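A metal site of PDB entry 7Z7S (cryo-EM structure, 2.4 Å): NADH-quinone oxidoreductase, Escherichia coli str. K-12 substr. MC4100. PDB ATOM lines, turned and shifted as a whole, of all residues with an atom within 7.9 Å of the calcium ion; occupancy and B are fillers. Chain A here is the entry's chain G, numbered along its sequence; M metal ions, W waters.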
ATOM      1  N   GLU A 615     -12.619 -17.552 -19.176  1.00  0.00           N
ATOM      2  CA  GLU A 615     -11.935 -18.814 -19.402  1.00  0.00           C
ATOM      3  C   GLU A 615     -12.774 -20.016 -18.990  1.00  0.00           C
ATOM      4  O   GLU A 615     -12.234 -21.102 -18.793  1.00  0.00           O
ATOM      5  CB  GLU A 615     -10.596 -18.829 -18.682  1.00  0.00           C
ATOM      6  CG  GLU A 615      -9.728 -17.641 -18.994  1.00  0.00           C
ATOM      7  CD  GLU A 615      -9.480 -16.759 -17.807  1.00  0.00           C
ATOM      8  OE1 GLU A 615     -10.171 -16.924 -16.779  1.00  0.00           O
ATOM      9  OE2 GLU A 615      -8.602 -15.883 -17.887  1.00  0.00           O
ATOM     10  N   SER A 616     -14.082 -19.851 -18.882  1.00  0.00           N
ATOM     11  CA  SER A 616     -14.948 -20.922 -18.423  1.00  0.00           C
ATOM     12  C   SER A 616     -16.263 -20.904 -19.192  1.00  0.00           C
ATOM     13  O   SER A 616     -16.635 -19.905 -19.797  1.00  0.00           O
ATOM     14  CB  SER A 616     -15.231 -20.812 -16.925  1.00  0.00           C
ATOM     15  OG  SER A 616     -16.000 -19.670 -16.622  1.00  0.00           O
ATOM     16  N   ASP A 617     -16.946 -22.029 -19.147  1.00  0.00           N
ATOM     17  CA  ASP A 617     -18.302 -22.161 -19.660  1.00  0.00           C
ATOM     18  C   ASP A 617     -19.221 -22.428 -18.480  1.00  0.00           C
ATOM     19  O   ASP A 617     -18.797 -23.000 -17.473  1.00  0.00           O
ATOM     20  CB  ASP A 617     -18.412 -23.288 -20.675  1.00  0.00           C
ATOM     21  CG  ASP A 617     -17.239 -23.345 -21.602  1.00  0.00           C
ATOM     22  OD1 ASP A 617     -16.199 -23.887 -21.188  1.00  0.00           O
ATOM     23  OD2 ASP A 617     -17.331 -22.837 -22.740  1.00  0.00           O
ATOM     24  N   GLY A 618     -20.470 -22.016 -18.596  1.00  0.00           N
ATOM     25  CA  GLY A 618     -21.386 -22.273 -17.512  1.00  0.00           C
ATOM     26  C   GLY A 618     -22.737 -21.667 -17.798  1.00  0.00           C
ATOM     27  O   GLY A 618     -22.997 -21.143 -18.882  1.00  0.00           O
ATOM     28  N   PHE A 631     -20.018 -18.884 -22.641  1.00  0.00           N
ATOM     29  CA  PHE A 631     -19.046 -19.758 -23.281  1.00  0.00           C
ATOM     30  C   PHE A 631     -17.652 -19.214 -23.037  1.00  0.00           C
ATOM     31  O   PHE A 631     -17.465 -18.014 -22.835  1.00  0.00           O
ATOM     32  CB  PHE A 631     -19.321 -19.857 -24.784  1.00  0.00           C
ATOM     33  CG  PHE A 631     -20.672 -20.413 -25.133  1.00  0.00           C
ATOM     34  CD1 PHE A 631     -21.797 -19.605 -25.116  1.00  0.00           C
ATOM     35  CD2 PHE A 631     -20.817 -21.728 -25.489  1.00  0.00           C
ATOM     36  CE1 PHE A 631     -23.028 -20.111 -25.441  1.00  0.00           C
ATOM     37  CE2 PHE A 631     -22.048 -22.242 -25.809  1.00  0.00           C
ATOM     38  CZ  PHE A 631     -23.154 -21.429 -25.787  1.00  0.00           C
ATOM     39  N   GLN A 632     -16.686 -20.125 -23.037  1.00  0.00           N
ATOM     40  CA  GLN A 632     -15.297 -19.744 -22.851  1.00  0.00           C
ATOM     41  C   GLN A 632     -14.805 -18.903 -24.020  1.00  0.00           C
ATOM     42  O   GLN A 632     -15.115 -19.185 -25.179  1.00  0.00           O
ATOM     43  CB  GLN A 632     -14.428 -21.001 -22.705  1.00  0.00           C
ATOM     44  CG  GLN A 632     -12.977 -20.737 -22.432  1.00  0.00           C
ATOM     45  CD  GLN A 632     -12.233 -21.976 -22.007  1.00  0.00           C
ATOM     46  OE1 GLN A 632     -12.842 -23.001 -21.710  1.00  0.00           O
ATOM     47  NE2 GLN A 632     -10.917 -21.888 -21.966  1.00  0.00           N
ATOM     48  N   VAL A 633     -14.048 -17.854 -23.713  1.00  0.00           N
ATOM     49  CA  VAL A 633     -13.530 -16.967 -24.751  1.00  0.00           C
ATOM     50  C   VAL A 633     -12.214 -17.480 -25.320  1.00  0.00           C
ATOM     51  O   VAL A 633     -12.024 -17.540 -26.529  1.00  0.00           O
ATOM     52  CB  VAL A 633     -13.383 -15.536 -24.202  1.00  0.00           C
ATOM     53  CG1 VAL A 633     -13.130 -14.563 -25.336  1.00  0.00           C
ATOM     54  CG2 VAL A 633     -14.623 -15.150 -23.433  1.00  0.00           C
ATOM     55  N   TYR A 634     -11.296 -17.882 -24.447  1.00  0.00           N
ATOM     56  CA  TYR A 634      -9.982 -18.279 -24.892  1.00  0.00           C
ATOM     57  C   TYR A 634      -9.445 -19.353 -23.959  1.00  0.00           C
ATOM     58  O   TYR A 634      -9.945 -19.544 -22.856  1.00  0.00           O
ATOM     59  CB  TYR A 634      -9.011 -17.090 -24.956  1.00  0.00           C
ATOM     60  CG  TYR A 634      -8.646 -16.528 -23.607  1.00  0.00           C
ATOM     61  CD1 TYR A 634      -9.528 -15.726 -22.912  1.00  0.00           C
ATOM     62  CD2 TYR A 634      -7.410 -16.808 -23.033  1.00  0.00           C
ATOM     63  CE1 TYR A 634      -9.202 -15.216 -21.683  1.00  0.00           C
ATOM     64  CE2 TYR A 634      -7.081 -16.302 -21.812  1.00  0.00           C
ATOM     65  CZ  TYR A 634      -7.966 -15.501 -21.141  1.00  0.00           C
ATOM     66  OH  TYR A 634      -7.649 -14.994 -19.915  1.00  0.00           O
ATOM     67  N   ASP A 635      -8.420 -20.046 -24.425  1.00  0.00           N
ATOM     68  CA  ASP A 635      -7.712 -21.005 -23.601  1.00  0.00           C
ATOM     69  C   ASP A 635      -6.512 -20.322 -22.949  1.00  0.00           C
ATOM     70  O   ASP A 635      -5.613 -19.864 -23.663  1.00  0.00           O
ATOM     71  CB  ASP A 635      -7.247 -22.180 -24.439  1.00  0.00           C
ATOM     72  CG  ASP A 635      -6.592 -23.260 -23.618  1.00  0.00           C
ATOM     73  OD1 ASP A 635      -7.163 -23.637 -22.578  1.00  0.00           O
ATOM     74  OD2 ASP A 635      -5.509 -23.729 -24.008  1.00  0.00           O
ATOM     75  N   LEU A 646      -8.669 -24.001 -14.609  1.00  0.00           N
ATOM     76  CA  LEU A 646      -9.763 -24.826 -15.076  1.00  0.00           C
ATOM     77  C   LEU A 646     -11.090 -24.243 -14.613  1.00  0.00           C
ATOM     78  O   LEU A 646     -11.148 -23.384 -13.733  1.00  0.00           O
ATOM     79  CB  LEU A 646      -9.627 -26.270 -14.581  1.00  0.00           C
ATOM     80  CG  LEU A 646      -8.384 -27.006 -15.058  1.00  0.00           C
ATOM     81  CD1 LEU A 646      -8.326 -28.373 -14.430  1.00  0.00           C
ATOM     82  CD2 LEU A 646      -8.387 -27.114 -16.566  1.00  0.00           C
ATOM     83  N   GLU A 647     -12.162 -24.715 -15.236  1.00  0.00           N
ATOM     84  CA  GLU A 647     -13.494 -24.406 -14.759  1.00  0.00           C
ATOM     85  C   GLU A 647     -13.676 -24.960 -13.362  1.00  0.00           C
ATOM     86  O   GLU A 647     -13.112 -25.992 -12.993  1.00  0.00           O
ATOM     87  CB  GLU A 647     -14.552 -25.006 -15.693  1.00  0.00           C
ATOM     88  CG  GLU A 647     -14.615 -24.370 -17.061  1.00  0.00           C
ATOM     89  CD  GLU A 647     -13.755 -25.068 -18.088  1.00  0.00           C
ATOM     90  OE1 GLU A 647     -12.770 -25.732 -17.701  1.00  0.00           O
ATOM     91  OE2 GLU A 647     -14.057 -24.960 -19.274  1.00  0.00           O
ATOM     92  N   TRP A 649     -16.389 -26.165 -11.950  1.00  0.00           N
ATOM     93  CA  TRP A 649     -17.092 -27.448 -11.948  1.00  0.00           C
ATOM     94  C   TRP A 649     -16.180 -28.575 -12.398  1.00  0.00           C
ATOM     95  O   TRP A 649     -16.335 -29.703 -11.934  1.00  0.00           O
ATOM     96  CB  TRP A 649     -18.334 -27.379 -12.839  1.00  0.00           C
ATOM     97  CG  TRP A 649     -18.105 -26.799 -14.195  1.00  0.00           C
ATOM     98  CD1 TRP A 649     -18.272 -25.498 -14.559  1.00  0.00           C
ATOM     99  CD2 TRP A 649     -17.668 -27.492 -15.368  1.00  0.00           C
ATOM    100  NE1 TRP A 649     -17.972 -25.338 -15.878  1.00  0.00           N
ATOM    101  CE2 TRP A 649     -17.596 -26.549 -16.398  1.00  0.00           C
ATOM    102  CE3 TRP A 649     -17.351 -28.815 -15.642  1.00  0.00           C
ATOM    103  CZ2 TRP A 649     -17.202 -26.888 -17.684  1.00  0.00           C
ATOM    104  CZ3 TRP A 649     -16.951 -29.147 -16.917  1.00  0.00           C
ATOM    105  CH2 TRP A 649     -16.876 -28.195 -17.927  1.00  0.00           C
ATOM    106  N   ARG A 650     -15.210 -28.288 -13.276  1.00  0.00           N
ATOM    107  CA  ARG A 650     -14.238 -29.292 -13.674  1.00  0.00           C
ATOM    108  C   ARG A 650     -13.350 -29.687 -12.503  1.00  0.00           C
ATOM    109  O   ARG A 650     -13.140 -30.880 -12.250  1.00  0.00           O
ATOM    110  CB  ARG A 650     -13.410 -28.776 -14.846  1.00  0.00           C
ATOM    111  CG  ARG A 650     -12.333 -29.719 -15.334  1.00  0.00           C
ATOM    112  CD  ARG A 650     -11.954 -29.422 -16.762  1.00  0.00           C
ATOM    113  NE  ARG A 650     -12.839 -30.096 -17.711  1.00  0.00           N
ATOM    114  CZ  ARG A 650     -13.433 -29.510 -18.734  1.00  0.00           C
ATOM    115  NH1 ARG A 650     -13.266 -28.224 -18.971  1.00  0.00           N
ATOM    116  NH2 ARG A 650     -14.218 -30.230 -19.531  1.00  0.00           N
ATOM    117  N   LEU A 669     -18.787 -30.452 -20.089  1.00  0.00           N
ATOM    118  CA  LEU A 669     -19.790 -29.531 -19.575  1.00  0.00           C
ATOM    119  C   LEU A 669     -21.197 -30.133 -19.636  1.00  0.00           C
ATOM    120  O   LEU A 669     -21.958 -30.020 -18.663  1.00  0.00           O
ATOM    121  CB  LEU A 669     -19.745 -28.206 -20.341  1.00  0.00           C
ATOM    122  CG  LEU A 669     -20.910 -27.246 -20.093  1.00  0.00           C
ATOM    123  CD1 LEU A 669     -20.872 -26.688 -18.685  1.00  0.00           C
ATOM    124  CD2 LEU A 669     -20.905 -26.113 -21.104  1.00  0.00           C
ATOM    125  N   ARG A 704     -15.068 -18.767 -33.203  1.00  0.00           N
ATOM    126  CA  ARG A 704     -14.855 -17.770 -32.160  1.00  0.00           C
ATOM    127  C   ARG A 704     -14.138 -16.531 -32.670  1.00  0.00           C
ATOM    128  O   ARG A 704     -14.153 -15.499 -32.000  1.00  0.00           O
ATOM    129  CB  ARG A 704     -14.049 -18.354 -31.009  1.00  0.00           C
ATOM    130  CG  ARG A 704     -14.870 -19.002 -29.927  1.00  0.00           C
ATOM    131  CD  ARG A 704     -14.010 -19.266 -28.708  1.00  0.00           C
ATOM    132  NE  ARG A 704     -14.737 -19.931 -27.639  1.00  0.00           N
ATOM    133  CZ  ARG A 704     -14.849 -21.248 -27.529  1.00  0.00           C
ATOM    134  NH1 ARG A 704     -14.328 -22.070 -28.416  1.00  0.00           N
ATOM    135  NH2 ARG A 704     -15.504 -21.751 -26.491  1.00  0.00           N
ATOM    136  N   GLN A 728      -8.488 -27.222 -28.153  1.00  0.00           N
ATOM    137  CA  GLN A 728      -9.713 -27.929 -28.457  1.00  0.00           C
ATOM    138  C   GLN A 728     -10.797 -27.542 -27.476  1.00  0.00           C
ATOM    139  O   GLN A 728     -10.530 -27.271 -26.305  1.00  0.00           O
ATOM    140  CB  GLN A 728      -9.477 -29.436 -28.416  1.00  0.00           C
ATOM    141  CG  GLN A 728      -8.520 -29.922 -29.497  1.00  0.00           C
ATOM    142  CD  GLN A 728      -8.993 -29.532 -30.885  1.00  0.00           C
ATOM    143  OE1 GLN A 728      -9.965 -30.093 -31.396  1.00  0.00           O
ATOM    144  NE2 GLN A 728      -8.324 -28.571 -31.491  1.00  0.00           N
ATOM    145  N   ASP A 729     -12.034 -27.503 -27.969  1.00  0.00           N
ATOM    146  CA  ASP A 729     -13.199 -27.199 -27.158  1.00  0.00           C
ATOM    147  C   ASP A 729     -14.103 -28.430 -27.177  1.00  0.00           C
ATOM    148  O   ASP A 729     -14.955 -28.575 -28.064  1.00  0.00           O
ATOM    149  CB  ASP A 729     -13.917 -25.973 -27.660  1.00  0.00           C
ATOM    150  CG  ASP A 729     -14.966 -25.465 -26.695  1.00  0.00           C
ATOM    151  OD1 ASP A 729     -15.021 -25.948 -25.556  1.00  0.00           O
ATOM    152  OD2 ASP A 729     -15.740 -24.564 -27.067  1.00  0.00           O
ATOM    153  N   ILE A 730     -13.919 -29.317 -26.197  1.00  0.00           N
ATOM    154  CA  ILE A 730     -14.835 -30.444 -26.046  1.00  0.00           C
ATOM    155  C   ILE A 730     -16.084 -30.061 -25.279  1.00  0.00           C
ATOM    156  O   ILE A 730     -17.047 -30.835 -25.265  1.00  0.00           O
ATOM    157  CB  ILE A 730     -14.153 -31.628 -25.332  1.00  0.00           C
ATOM    158  CG1 ILE A 730     -13.920 -31.296 -23.866  1.00  0.00           C
ATOM    159  CG2 ILE A 730     -12.852 -31.974 -26.014  1.00  0.00           C
ATOM    160  CD1 ILE A 730     -13.626 -32.492 -23.022  1.00  0.00           C
ATOM    161  N   ASP A 731     -16.109 -28.884 -24.676  1.00  0.00           N
ATOM    162  CA  ASP A 731     -17.207 -28.510 -23.787  1.00  0.00           C
ATOM    163  C   ASP A 731     -18.400 -27.951 -24.558  1.00  0.00           C
ATOM    164  O   ASP A 731     -19.546 -28.189 -24.176  1.00  0.00           O
ATOM    165  CB  ASP A 731     -16.728 -27.501 -22.749  1.00  0.00           C
ATOM    166  CG  ASP A 731     -15.813 -28.121 -21.725  1.00  0.00           C
ATOM    167  OD1 ASP A 731     -16.150 -29.211 -21.222  1.00  0.00           O
ATOM    168  OD2 ASP A 731     -14.764 -27.531 -21.405  1.00  0.00           O
ATOM    169  N   THR A 732     -18.162 -27.172 -25.602  1.00  0.00           N
ATOM    170  CA  THR A 732     -19.225 -26.457 -26.298  1.00  0.00           C
ATOM    171  C   THR A 732     -19.110 -26.649 -27.804  1.00  0.00           C
ATOM    172  O   THR A 732     -18.202 -27.309 -28.307  1.00  0.00           O
ATOM    173  CB  THR A 732     -19.219 -24.953 -25.974  1.00  0.00           C
ATOM    174  OG1 THR A 732     -18.019 -24.352 -26.480  1.00  0.00           O
ATOM    175  CG2 THR A 732     -19.310 -24.717 -24.478  1.00  0.00           C
ATOM    176  N   PHE A 736     -12.097 -22.894 -31.096  1.00  0.00           N
ATOM    177  CA  PHE A 736     -11.112 -21.858 -30.787  1.00  0.00           C
ATOM    178  C   PHE A 736     -10.304 -21.478 -32.024  1.00  0.00           C
ATOM    179  O   PHE A 736      -9.076 -21.502 -31.981  1.00  0.00           O
ATOM    180  CB  PHE A 736     -10.159 -22.338 -29.692  1.00  0.00           C
ATOM    181  CG  PHE A 736     -10.756 -22.323 -28.323  1.00  0.00           C
ATOM    182  CD1 PHE A 736     -11.013 -21.139 -27.663  1.00  0.00           C
ATOM    183  CD2 PHE A 736     -11.051 -23.516 -27.677  1.00  0.00           C
ATOM    184  CE1 PHE A 736     -11.546 -21.134 -26.403  1.00  0.00           C
ATOM    185  CE2 PHE A 736     -11.592 -23.514 -26.419  1.00  0.00           C
ATOM    186  CZ  PHE A 736     -11.838 -22.323 -25.770  1.00  0.00           C
HETATM  187 CA    CA M   1     -14.165 -25.105 -21.724  1.00  0.00          CA
HETATM  188  O   HOH W   1     -11.727 -25.813 -21.741  1.00  0.00           O
HETATM  189  O   HOH W   2     -15.224 -24.195 -23.905  1.00  0.00           O
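The backbone carbonyl oxygen (O) of Asp 617 sits at hydrogen-bond distance from the indole nitrogen (NE1) of Trp 649 (2.9 Å). NH1 of Arg 650 lies within salt-bridge range of OE1 of Glu 647. The backbone NH (N) of Gln 632 sits at hydrogen-bond distance from the backbone carbonyl oxygen (O) of Ser 616 (3.2 Å). The backbone carbonyl oxygen (O) of Gln 632 is in hydrogen-bond range of the guanidinium group (NE) of Arg 704 (2.6 Å). O of Tyr 634 sits at hydrogen-bond distance from NE2 of Gln 632. OD1 of Asp 729 sits close to N of Asp 731 (3.3 Å). OD1 of Asp 731 lies within salt-bridge range of NH2 of Arg 650, 2.8 Å away. The side-chain carboxylate (OD1) of Asp 731 lies within hydrogen-bond range of the backbone NH (N) of Leu 669 (3.1 Å).
Of the 21 residues printed, 4 come within 4 Å of the calcium ion.
The calcium ion is bound by OD1 of Asp 617 (2.4 Å), OE2 of Glu 647 (2.5 Å), OE1 of Gln 632 (2.5 Å), OD2 of Asp 731 (2.5 Å), water W1 (2.5 Å) and water W2 (2.6 Å).
Water W2 bridges the side-chain carboxylate of Asp 729 (2.4 Å) and the side-chain carboxylate of Asp 617 (2.8 Å).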
